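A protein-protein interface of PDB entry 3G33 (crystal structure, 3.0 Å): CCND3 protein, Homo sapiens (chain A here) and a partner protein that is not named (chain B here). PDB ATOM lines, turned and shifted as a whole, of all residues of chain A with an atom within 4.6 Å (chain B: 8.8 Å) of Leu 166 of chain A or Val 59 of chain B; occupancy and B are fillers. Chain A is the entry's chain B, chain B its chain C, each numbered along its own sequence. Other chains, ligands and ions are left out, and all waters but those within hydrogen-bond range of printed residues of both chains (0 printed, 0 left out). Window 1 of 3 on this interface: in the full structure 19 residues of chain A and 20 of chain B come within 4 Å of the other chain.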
ATOM      1  N   LEU A  94     -19.074 -21.418   4.052  1.00  0.00           N
ATOM      2  CA  LEU A  94     -17.918 -20.576   3.789  1.00  0.00           C
ATOM      3  C   LEU A  94     -16.950 -20.670   4.963  1.00  0.00           C
ATOM      4  O   LEU A  94     -15.747 -20.849   4.777  1.00  0.00           O
ATOM      5  CB  LEU A  94     -18.356 -19.127   3.581  1.00  0.00           C
ATOM      6  CG  LEU A  94     -17.638 -18.332   2.488  1.00  0.00           C
ATOM      7  CD1 LEU A  94     -17.875 -16.841   2.672  1.00  0.00           C
ATOM      8  CD2 LEU A  94     -16.151 -18.638   2.481  1.00  0.00           C
ATOM      9  N   TYR A  98     -12.991 -21.994   5.142  1.00  0.00           N
ATOM     10  CA  TYR A  98     -11.833 -21.393   5.787  1.00  0.00           C
ATOM     11  C   TYR A  98     -11.188 -22.388   6.742  1.00  0.00           C
ATOM     12  O   TYR A  98      -9.969 -22.558   6.749  1.00  0.00           O
ATOM     13  CB  TYR A  98     -12.227 -20.123   6.543  1.00  0.00           C
ATOM     14  CG  TYR A  98     -12.878 -19.063   5.681  1.00  0.00           C
ATOM     15  CD1 TYR A  98     -12.568 -18.950   4.333  1.00  0.00           C
ATOM     16  CD2 TYR A  98     -13.785 -18.160   6.224  1.00  0.00           C
ATOM     17  CE1 TYR A  98     -13.156 -17.979   3.543  1.00  0.00           C
ATOM     18  CE2 TYR A  98     -14.377 -17.185   5.443  1.00  0.00           C
ATOM     19  CZ  TYR A  98     -14.058 -17.100   4.103  1.00  0.00           C
ATOM     20  OH  TYR A  98     -14.644 -16.132   3.321  1.00  0.00           O
ATOM     21  N   LEU A 123     -15.125 -14.107   9.957  1.00  0.00           N
ATOM     22  CA  LEU A 123     -14.686 -13.751   8.613  1.00  0.00           C
ATOM     23  C   LEU A 123     -15.767 -14.031   7.573  1.00  0.00           C
ATOM     24  O   LEU A 123     -16.164 -13.138   6.823  1.00  0.00           O
ATOM     25  CB  LEU A 123     -13.399 -14.497   8.254  1.00  0.00           C
ATOM     26  CG  LEU A 123     -12.137 -14.054   8.999  1.00  0.00           C
ATOM     27  CD1 LEU A 123     -10.994 -15.024   8.749  1.00  0.00           C
ATOM     28  CD2 LEU A 123     -11.742 -12.640   8.598  1.00  0.00           C
ATOM     29  N   LEU A 127     -17.691 -11.151   5.240  1.00  0.00           N
ATOM     30  CA  LEU A 127     -17.495 -11.100   3.800  1.00  0.00           C
ATOM     31  C   LEU A 127     -18.807 -11.175   3.029  1.00  0.00           C
ATOM     32  O   LEU A 127     -18.892 -10.701   1.897  1.00  0.00           O
ATOM     33  CB  LEU A 127     -16.572 -12.232   3.350  1.00  0.00           C
ATOM     34  CG  LEU A 127     -15.890 -12.035   1.997  1.00  0.00           C
ATOM     35  CD1 LEU A 127     -14.680 -11.127   2.144  1.00  0.00           C
ATOM     36  CD2 LEU A 127     -15.482 -13.372   1.402  1.00  0.00           C
ATOM     37  N   LEU A 159      -6.314 -14.827   8.420  1.00  0.00           N
ATOM     38  CA  LEU A 159      -6.250 -14.087   7.165  1.00  0.00           C
ATOM     39  C   LEU A 159      -4.903 -14.277   6.478  1.00  0.00           C
ATOM     40  O   LEU A 159      -4.840 -14.558   5.281  1.00  0.00           O
ATOM     41  CB  LEU A 159      -6.506 -12.598   7.404  1.00  0.00           C
ATOM     42  CG  LEU A 159      -7.965 -12.146   7.437  1.00  0.00           C
ATOM     43  CD1 LEU A 159      -8.077 -10.743   8.012  1.00  0.00           C
ATOM     44  CD2 LEU A 159      -8.572 -12.212   6.043  1.00  0.00           C
ATOM     45  N   LEU A 162      -4.405 -17.722   5.097  1.00  0.00           N
ATOM     46  CA  LEU A 162      -5.224 -17.927   3.910  1.00  0.00           C
ATOM     47  C   LEU A 162      -4.921 -16.850   2.878  1.00  0.00           C
ATOM     48  O   LEU A 162      -5.648 -16.691   1.897  1.00  0.00           O
ATOM     49  CB  LEU A 162      -6.709 -17.906   4.270  1.00  0.00           C
ATOM     50  CG  LEU A 162      -7.189 -18.974   5.252  1.00  0.00           C
ATOM     51  CD1 LEU A 162      -8.683 -18.828   5.518  1.00  0.00           C
ATOM     52  CD2 LEU A 162      -6.866 -20.365   4.730  1.00  0.00           C
ATOM     53  N   TRP A 164      -5.463 -13.849   2.809  1.00  0.00           N
ATOM     54  CA  TRP A 164      -6.564 -12.912   2.611  1.00  0.00           C
ATOM     55  C   TRP A 164      -7.433 -13.279   1.412  1.00  0.00           C
ATOM     56  O   TRP A 164      -8.199 -12.453   0.919  1.00  0.00           O
ATOM     57  CB  TRP A 164      -6.031 -11.488   2.446  1.00  0.00           C
ATOM     58  CG  TRP A 164      -5.472 -10.899   3.703  1.00  0.00           C
ATOM     59  CD1 TRP A 164      -4.386 -11.339   4.402  1.00  0.00           C
ATOM     60  CD2 TRP A 164      -5.962  -9.751   4.404  1.00  0.00           C
ATOM     61  NE1 TRP A 164      -4.174 -10.541   5.499  1.00  0.00           N
ATOM     62  CE2 TRP A 164      -5.127  -9.557   5.523  1.00  0.00           C
ATOM     63  CE3 TRP A 164      -7.028  -8.869   4.197  1.00  0.00           C
ATOM     64  CZ2 TRP A 164      -5.325  -8.519   6.431  1.00  0.00           C
ATOM     65  CZ3 TRP A 164      -7.223  -7.840   5.099  1.00  0.00           C
ATOM     66  CH2 TRP A 164      -6.375  -7.672   6.201  1.00  0.00           C
ATOM     67  N   ASP A 165      -7.309 -14.515   0.941  1.00  0.00           N
ATOM     68  CA  ASP A 165      -8.124 -14.984  -0.173  1.00  0.00           C
ATOM     69  C   ASP A 165      -9.396 -15.639   0.357  1.00  0.00           C
ATOM     70  O   ASP A 165      -9.452 -16.856   0.527  1.00  0.00           O
ATOM     71  CB  ASP A 165      -7.334 -15.973  -1.028  1.00  0.00           C
ATOM     72  CG  ASP A 165      -7.956 -16.193  -2.392  1.00  0.00           C
ATOM     73  OD1 ASP A 165      -9.107 -15.753  -2.601  1.00  0.00           O
ATOM     74  OD2 ASP A 165      -7.294 -16.805  -3.256  1.00  0.00           O
ATOM     75  N   LEU A 166     -10.417 -14.827   0.610  1.00  0.00           N
ATOM     76  CA  LEU A 166     -11.627 -15.311   1.273  1.00  0.00           C
ATOM     77  C   LEU A 166     -12.868 -15.291   0.383  1.00  0.00           C
ATOM     78  O   LEU A 166     -13.898 -15.864   0.738  1.00  0.00           O
ATOM     79  CB  LEU A 166     -11.891 -14.508   2.551  1.00  0.00           C
ATOM     80  CG  LEU A 166     -10.755 -14.476   3.578  1.00  0.00           C
ATOM     81  CD1 LEU A 166     -11.110 -13.565   4.742  1.00  0.00           C
ATOM     82  CD2 LEU A 166     -10.435 -15.881   4.068  1.00  0.00           C
ATOM     83  N   ALA A 167     -12.773 -14.627  -0.764  1.00  0.00           N
ATOM     84  CA  ALA A 167     -13.885 -14.579  -1.708  1.00  0.00           C
ATOM     85  C   ALA A 167     -14.030 -15.922  -2.413  1.00  0.00           C
ATOM     86  O   ALA A 167     -14.066 -15.991  -3.640  1.00  0.00           O
ATOM     87  CB  ALA A 167     -13.678 -13.467  -2.720  1.00  0.00           C
ATOM     88  N   ALA A 168     -14.116 -16.985  -1.622  1.00  0.00           N
ATOM     89  CA  ALA A 168     -14.144 -18.343  -2.149  1.00  0.00           C
ATOM     90  C   ALA A 168     -15.483 -18.702  -2.778  1.00  0.00           C
ATOM     91  O   ALA A 168     -16.527 -18.173  -2.396  1.00  0.00           O
ATOM     92  CB  ALA A 168     -13.796 -19.338  -1.055  1.00  0.00           C
ATOM     93  N   VAL B  44      -4.204  -0.488   9.179  1.00  0.00           N
ATOM     94  CA  VAL B  44      -5.646  -0.750   9.292  1.00  0.00           C
ATOM     95  C   VAL B  44      -6.181  -0.719  10.727  1.00  0.00           C
ATOM     96  O   VAL B  44      -5.409  -0.611  11.680  1.00  0.00           O
ATOM     97  CB  VAL B  44      -6.012  -2.116   8.677  1.00  0.00           C
ATOM     98  CG1 VAL B  44      -7.492  -2.403   8.866  1.00  0.00           C
ATOM     99  CG2 VAL B  44      -5.641  -2.151   7.203  1.00  0.00           C
ATOM    100  N   PRO B  45      -7.514  -0.815  10.882  1.00  0.00           N
ATOM    101  CA  PRO B  45      -8.148  -0.884  12.203  1.00  0.00           C
ATOM    102  C   PRO B  45      -8.048  -2.279  12.825  1.00  0.00           C
ATOM    103  O   PRO B  45      -8.450  -3.265  12.203  1.00  0.00           O
ATOM    104  CB  PRO B  45      -9.618  -0.533  11.920  1.00  0.00           C
ATOM    105  CG  PRO B  45      -9.696  -0.170  10.452  1.00  0.00           C
ATOM    106  CD  PRO B  45      -8.509  -0.798   9.796  1.00  0.00           C
ATOM    107  N   GLY B  53     -12.574  -5.536  16.176  1.00  0.00           N
ATOM    108  CA  GLY B  53     -13.148  -5.821  14.874  1.00  0.00           C
ATOM    109  C   GLY B  53     -12.228  -5.436  13.736  1.00  0.00           C
ATOM    110  O   GLY B  53     -11.288  -4.660  13.911  1.00  0.00           O
ATOM    111  N   LEU B  54     -12.502  -5.994  12.565  1.00  0.00           N
ATOM    112  CA  LEU B  54     -11.790  -5.624  11.363  1.00  0.00           C
ATOM    113  C   LEU B  54     -12.752  -4.937  10.421  1.00  0.00           C
ATOM    114  O   LEU B  54     -13.936  -5.273  10.374  1.00  0.00           O
ATOM    115  CB  LEU B  54     -11.181  -6.852  10.691  1.00  0.00           C
ATOM    116  CG  LEU B  54     -10.005  -7.483  11.436  1.00  0.00           C
ATOM    117  CD1 LEU B  54      -9.449  -8.670  10.662  1.00  0.00           C
ATOM    118  CD2 LEU B  54      -8.918  -6.447  11.684  1.00  0.00           C
ATOM    119  N   PRO B  55     -12.244  -3.963   9.664  1.00  0.00           N
ATOM    120  CA  PRO B  55     -13.128  -3.248   8.769  1.00  0.00           C
ATOM    121  C   PRO B  55     -13.548  -4.162   7.636  1.00  0.00           C
ATOM    122  O   PRO B  55     -12.742  -4.527   6.779  1.00  0.00           O
ATOM    123  CB  PRO B  55     -12.281  -2.078   8.264  1.00  0.00           C
ATOM    124  CG  PRO B  55     -10.881  -2.381   8.625  1.00  0.00           C
ATOM    125  CD  PRO B  55     -10.834  -3.563   9.537  1.00  0.00           C
ATOM    126  N   ILE B  56     -14.815  -4.541   7.664  1.00  0.00           N
ATOM    127  CA  ILE B  56     -15.379  -5.415   6.662  1.00  0.00           C
ATOM    128  C   ILE B  56     -14.966  -4.970   5.267  1.00  0.00           C
ATOM    129  O   ILE B  56     -14.566  -5.787   4.439  1.00  0.00           O
ATOM    130  CB  ILE B  56     -16.909  -5.430   6.771  1.00  0.00           C
ATOM    131  CG1 ILE B  56     -17.315  -5.842   8.195  1.00  0.00           C
ATOM    132  CG2 ILE B  56     -17.513  -6.383   5.733  1.00  0.00           C
ATOM    133  CD1 ILE B  56     -18.801  -5.762   8.465  1.00  0.00           C
ATOM    134  N   SER B  57     -15.054  -3.668   5.009  1.00  0.00           N
ATOM    135  CA  SER B  57     -14.775  -3.141   3.676  1.00  0.00           C
ATOM    136  C   SER B  57     -13.342  -3.430   3.233  1.00  0.00           C
ATOM    137  O   SER B  57     -13.072  -3.563   2.035  1.00  0.00           O
ATOM    138  CB  SER B  57     -15.055  -1.636   3.607  1.00  0.00           C
ATOM    139  OG  SER B  57     -13.935  -0.882   4.061  1.00  0.00           O
ATOM    140  N   THR B  58     -12.429  -3.530   4.195  1.00  0.00           N
ATOM    141  CA  THR B  58     -11.021  -3.783   3.890  1.00  0.00           C
ATOM    142  C   THR B  58     -10.749  -5.253   3.588  1.00  0.00           C
ATOM    143  O   THR B  58     -10.019  -5.580   2.649  1.00  0.00           O
ATOM    144  CB  THR B  58     -10.102  -3.353   5.046  1.00  0.00           C
ATOM    145  OG1 THR B  58     -10.241  -1.945   5.271  1.00  0.00           O
ATOM    146  CG2 THR B  58      -8.649  -3.666   4.709  1.00  0.00           C
ATOM    147  N   VAL B  59     -11.333  -6.133   4.395  1.00  0.00           N
ATOM    148  CA  VAL B  59     -11.156  -7.568   4.220  1.00  0.00           C
ATOM    149  C   VAL B  59     -11.811  -8.024   2.923  1.00  0.00           C
ATOM    150  O   VAL B  59     -11.355  -8.972   2.282  1.00  0.00           O
ATOM    151  CB  VAL B  59     -11.757  -8.359   5.402  1.00  0.00           C
ATOM    152  CG1 VAL B  59     -11.781  -9.857   5.098  1.00  0.00           C
ATOM    153  CG2 VAL B  59     -10.978  -8.078   6.681  1.00  0.00           C
ATOM    154  N   ARG B  60     -12.883  -7.336   2.541  1.00  0.00           N
ATOM    155  CA  ARG B  60     -13.596  -7.649   1.310  1.00  0.00           C
ATOM    156  C   ARG B  60     -12.784  -7.265   0.078  1.00  0.00           C
ATOM    157  O   ARG B  60     -12.563  -8.087  -0.809  1.00  0.00           O
ATOM    158  CB  ARG B  60     -14.959  -6.953   1.280  1.00  0.00           C
ATOM    159  CG  ARG B  60     -16.013  -7.617   2.148  1.00  0.00           C
ATOM    160  CD  ARG B  60     -17.363  -6.934   1.997  1.00  0.00           C
ATOM    161  NE  ARG B  60     -18.385  -7.544   2.843  1.00  0.00           N
ATOM    162  CZ  ARG B  60     -19.612  -7.058   2.995  1.00  0.00           C
ATOM    163  NH1 ARG B  60     -19.970  -5.951   2.359  1.00  0.00           N
ATOM    164  NH2 ARG B  60     -20.480  -7.675   3.785  1.00  0.00           N
ATOM    165  N   GLU B  61     -12.337  -6.015   0.028  1.00  0.00           N
ATOM    166  CA  GLU B  61     -11.610  -5.520  -1.137  1.00  0.00           C
ATOM    167  C   GLU B  61     -10.254  -6.198  -1.325  1.00  0.00           C
ATOM    168  O   GLU B  61      -9.794  -6.374  -2.453  1.00  0.00           O
ATOM    169  CB  GLU B  61     -11.454  -3.999  -1.079  1.00  0.00           C
ATOM    170  CG  GLU B  61     -12.746  -3.247  -1.356  1.00  0.00           C
ATOM    171  CD  GLU B  61     -12.534  -1.756  -1.533  1.00  0.00           C
ATOM    172  OE1 GLU B  61     -11.387  -1.345  -1.821  1.00  0.00           O
ATOM    173  OE2 GLU B  61     -13.515  -0.997  -1.389  1.00  0.00           O
ATOM    174  N   VAL B  62      -9.616  -6.580  -0.223  1.00  0.00           N
ATOM    175  CA  VAL B  62      -8.357  -7.311  -0.295  1.00  0.00           C
ATOM    176  C   VAL B  62      -8.606  -8.721  -0.815  1.00  0.00           C
ATOM    177  O   VAL B  62      -7.803  -9.268  -1.570  1.00  0.00           O
ATOM    178  CB  VAL B  62      -7.663  -7.391   1.075  1.00  0.00           C
ATOM    179  CG1 VAL B  62      -6.431  -8.277   0.993  1.00  0.00           C
ATOM    180  CG2 VAL B  62      -7.294  -6.001   1.565  1.00  0.00           C
ATOM    181  N   ALA B  63      -9.728  -9.303  -0.405  1.00  0.00           N
ATOM    182  CA  ALA B  63     -10.104 -10.638  -0.850  1.00  0.00           C
ATOM    183  C   ALA B  63     -10.582 -10.605  -2.296  1.00  0.00           C
ATOM    184  O   ALA B  63     -10.443 -11.584  -3.028  1.00  0.00           O
ATOM    185  CB  ALA B  63     -11.180 -11.214   0.054  1.00  0.00           C
ATOM    186  N   LEU B  64     -11.145  -9.473  -2.700  1.00  0.00           N
ATOM    187  CA  LEU B  64     -11.626  -9.305  -4.063  1.00  0.00           C
ATOM    188  C   LEU B  64     -10.457  -9.262  -5.038  1.00  0.00           C
ATOM    189  O   LEU B  64     -10.549  -9.771  -6.155  1.00  0.00           O
ATOM    190  CB  LEU B  64     -12.460  -8.029  -4.189  1.00  0.00           C
ATOM    191  CG  LEU B  64     -13.159  -7.811  -5.532  1.00  0.00           C
ATOM    192  CD1 LEU B  64     -14.140  -8.939  -5.814  1.00  0.00           C
ATOM    193  CD2 LEU B  64     -13.865  -6.464  -5.560  1.00  0.00           C
ATOM    194  N   LEU B  65      -9.359  -8.648  -4.610  1.00  0.00           N
ATOM    195  CA  LEU B  65      -8.147  -8.592  -5.422  1.00  0.00           C
ATOM    196  C   LEU B  65      -7.504  -9.967  -5.557  1.00  0.00           C
ATOM    197  O   LEU B  65      -7.188 -10.405  -6.662  1.00  0.00           O
ATOM    198  CB  LEU B  65      -7.148  -7.589  -4.840  1.00  0.00           C
ATOM    199  CG  LEU B  65      -7.163  -6.182  -5.444  1.00  0.00           C
ATOM    200  CD1 LEU B  65      -8.556  -5.793  -5.905  1.00  0.00           C
ATOM    201  CD2 LEU B  65      -6.615  -5.164  -4.456  1.00  0.00           C
ATOM    202  N   ARG B  66      -7.314 -10.648  -4.431  1.00  0.00           N
ATOM    203  CA  ARG B  66      -6.737 -11.987  -4.447  1.00  0.00           C
ATOM    204  C   ARG B  66      -7.492 -12.882  -5.426  1.00  0.00           C
ATOM    205  O   ARG B  66      -6.894 -13.708  -6.114  1.00  0.00           O
ATOM    206  CB  ARG B  66      -6.761 -12.604  -3.047  1.00  0.00           C
ATOM    207  CG  ARG B  66      -5.912 -11.868  -2.023  1.00  0.00           C
ATOM    208  CD  ARG B  66      -4.425 -12.143  -2.208  1.00  0.00           C
ATOM    209  NE  ARG B  66      -4.084 -13.536  -1.936  1.00  0.00           N
ATOM    210  CZ  ARG B  66      -3.574 -14.373  -2.834  1.00  0.00           C
ATOM    211  NH1 ARG B  66      -3.334 -13.957  -4.071  1.00  0.00           N
ATOM    212  NH2 ARG B  66      -3.296 -15.625  -2.495  1.00  0.00           N
ATOM    213  N   ARG B  67      -8.808 -12.706  -5.485  1.00  0.00           N
ATOM    214  CA  ARG B  67      -9.652 -13.506  -6.365  1.00  0.00           C
ATOM    215  C   ARG B  67      -9.270 -13.306  -7.829  1.00  0.00           C
ATOM    216  O   ARG B  67      -9.214 -14.264  -8.599  1.00  0.00           O
ATOM    217  CB  ARG B  67     -11.125 -13.157  -6.153  1.00  0.00           C
ATOM    218  CG  ARG B  67     -12.101 -14.143  -6.778  1.00  0.00           C
ATOM    219  CD  ARG B  67     -13.539 -13.721  -6.523  1.00  0.00           C
ATOM    220  NE  ARG B  67     -14.493 -14.749  -6.928  1.00  0.00           N
ATOM    221  CZ  ARG B  67     -15.812 -14.623  -6.827  1.00  0.00           C
ATOM    222  NH1 ARG B  67     -16.336 -13.509  -6.335  1.00  0.00           N
ATOM    223  NH2 ARG B  67     -16.608 -15.609  -7.221  1.00  0.00           N
ATOM    224  N   VAL B  82      -0.251 -11.496   0.962  1.00  0.00           N
ATOM    225  CA  VAL B  82      -0.688 -10.475   1.910  1.00  0.00           C
ATOM    226  C   VAL B  82      -0.122 -10.729   3.304  1.00  0.00           C
ATOM    227  O   VAL B  82      -0.327 -11.794   3.884  1.00  0.00           O
ATOM    228  CB  VAL B  82      -2.222 -10.400   1.998  1.00  0.00           C
ATOM    229  CG1 VAL B  82      -2.641  -9.323   2.984  1.00  0.00           C
ATOM    230  CG2 VAL B  82      -2.818 -10.133   0.627  1.00  0.00           C
ATOM    231  N   VAL B  94      -0.999  -3.737   7.205  1.00  0.00           N
ATOM    232  CA  VAL B  94      -1.208  -4.741   6.174  1.00  0.00           C
ATOM    233  C   VAL B  94      -0.308  -4.483   4.973  1.00  0.00           C
ATOM    234  O   VAL B  94      -0.362  -3.414   4.365  1.00  0.00           O
ATOM    235  CB  VAL B  94      -2.670  -4.759   5.701  1.00  0.00           C
ATOM    236  CG1 VAL B  94      -2.853  -5.772   4.582  1.00  0.00           C
ATOM    237  CG2 VAL B  94      -3.599  -5.061   6.867  1.00  0.00           C
ATOM    238  N   ARG B 168     -11.358   1.673  -0.617  1.00  0.00           N
ATOM    239  CA  ARG B 168     -11.686   1.713   0.805  1.00  0.00           C
ATOM    240  C   ARG B 168     -10.496   1.402   1.701  1.00  0.00           C
ATOM    241  O   ARG B 168     -10.571   1.542   2.923  1.00  0.00           O
ATOM    242  CB  ARG B 168     -12.859   0.784   1.117  1.00  0.00           C
ATOM    243  CG  ARG B 168     -14.195   1.497   1.069  1.00  0.00           C
ATOM    244  CD  ARG B 168     -15.356   0.530   0.985  1.00  0.00           C
ATOM    245  NE  ARG B 168     -16.612   1.205   1.290  1.00  0.00           N
ATOM    246  CZ  ARG B 168     -17.789   0.594   1.382  1.00  0.00           C
ATOM    247  NH1 ARG B 168     -17.878  -0.714   1.187  1.00  0.00           N
ATOM    248  NH2 ARG B 168     -18.879   1.294   1.669  1.00  0.00           N
ATOM    249  N   ILE B 169      -9.393   0.995   1.088  1.00  0.00           N
ATOM    250  CA  ILE B 169      -8.205   0.642   1.842  1.00  0.00           C
ATOM    251  C   ILE B 169      -7.343   1.873   2.101  1.00  0.00           C
ATOM    252  O   ILE B 169      -6.582   1.913   3.066  1.00  0.00           O
ATOM    253  CB  ILE B 169      -7.380  -0.423   1.106  1.00  0.00           C
ATOM    254  CG1 ILE B 169      -8.292  -1.273   0.218  1.00  0.00           C
ATOM    255  CG2 ILE B 169      -6.620  -1.286   2.103  1.00  0.00           C
ATOM    256  CD1 ILE B 169      -7.559  -2.327  -0.581  1.00  0.00           C
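NE of Arg 60 of chain B is in hydrogen-bond range of O of Leu 127 of chain A, at 3.3 Å.
The side-chain hydroxyl (OH) of Tyr 98 of chain A sits at hydrogen-bond distance from the backbone carbonyl oxygen (O) of Leu 166 of chain A (2.7 Å).
The backbone NH (N) of Trp 164 of chain A is in hydrogen-bond range of the backbone carbonyl oxygen (O) of Leu 159 of chain A, at 2.6 Å.
Leu 127 of chain A touches Val 59 of chain B.
CD1 of Leu 159 of chain A touches CD1 of Leu 54 of chain B (3.6 Å).
Trp 164 of chain A touches Ala 63 of chain B.
CG of Arg 66 of chain B touches O of Trp 164 of chain A (3.8 Å).
Trp 164 of chain A touches Val 94 of chain B (CH2 to CG2, 3.9 Å).
Arg 66 of chain B touches Asp 165 of chain A (CB to CG, 3.8 Å).
CG1 of Val 59 of chain B touches CD1 of Leu 166 of chain A, at 3.8 Å.
Leu 166 of chain A touches Ala 63 of chain B.
Ala 63 of chain B touches Ala 167 of chain A (O to CB, 3.8 Å).
NE of Arg 67 of chain B touches O of Ala 167 of chain A (3.5 Å).
Leu 166 of chain A touches just these residues of chain B: Val 59 and Ala 63.
Of chain A, only Leu 127 (3.96 Å) and Leu 166 (3.8 Å) come within 4 Å of Val 59 of chain B.
Printed residues of chain B within 4 Å of Leu 127 of chain A: Val 59 and Arg 60.
Of the printed residues of chain A, Ala 63 of chain B touches Trp 164 (3.2 Å), Leu 166 (3.7 Å) and Ala 167 (3.8 Å).
Printed residues of chain A within 4 Å of Val 82 of chain B: Trp 164 (3.0 Å).
Gly 53 of chain B touches none of the printed residues of chain A.
The nearest residue of chain A that does not touch Val 59 of chain B is Trp 164 of chain A (4.04 Å).
Printed residues of chain B that touch a printed residue of chain A: Leu 54, Val 59, Arg 60, Val 62, Ala 63, Arg 66, Arg 67, Val 82 and Val 94.
Hydrophobic or aromatic side chains of chain B that line the printed part of chain A: Leu 54, Val 59, Val 62, Ala 63, Val 82 and Val 94.
Of the 11 printed residues of chain A, 6 touch a printed residue of chain B.
Among the printed residues, no Asp or Glu carboxylate lies within 4 Å of a Lys or Arg side-chain nitrogen of the other chain.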
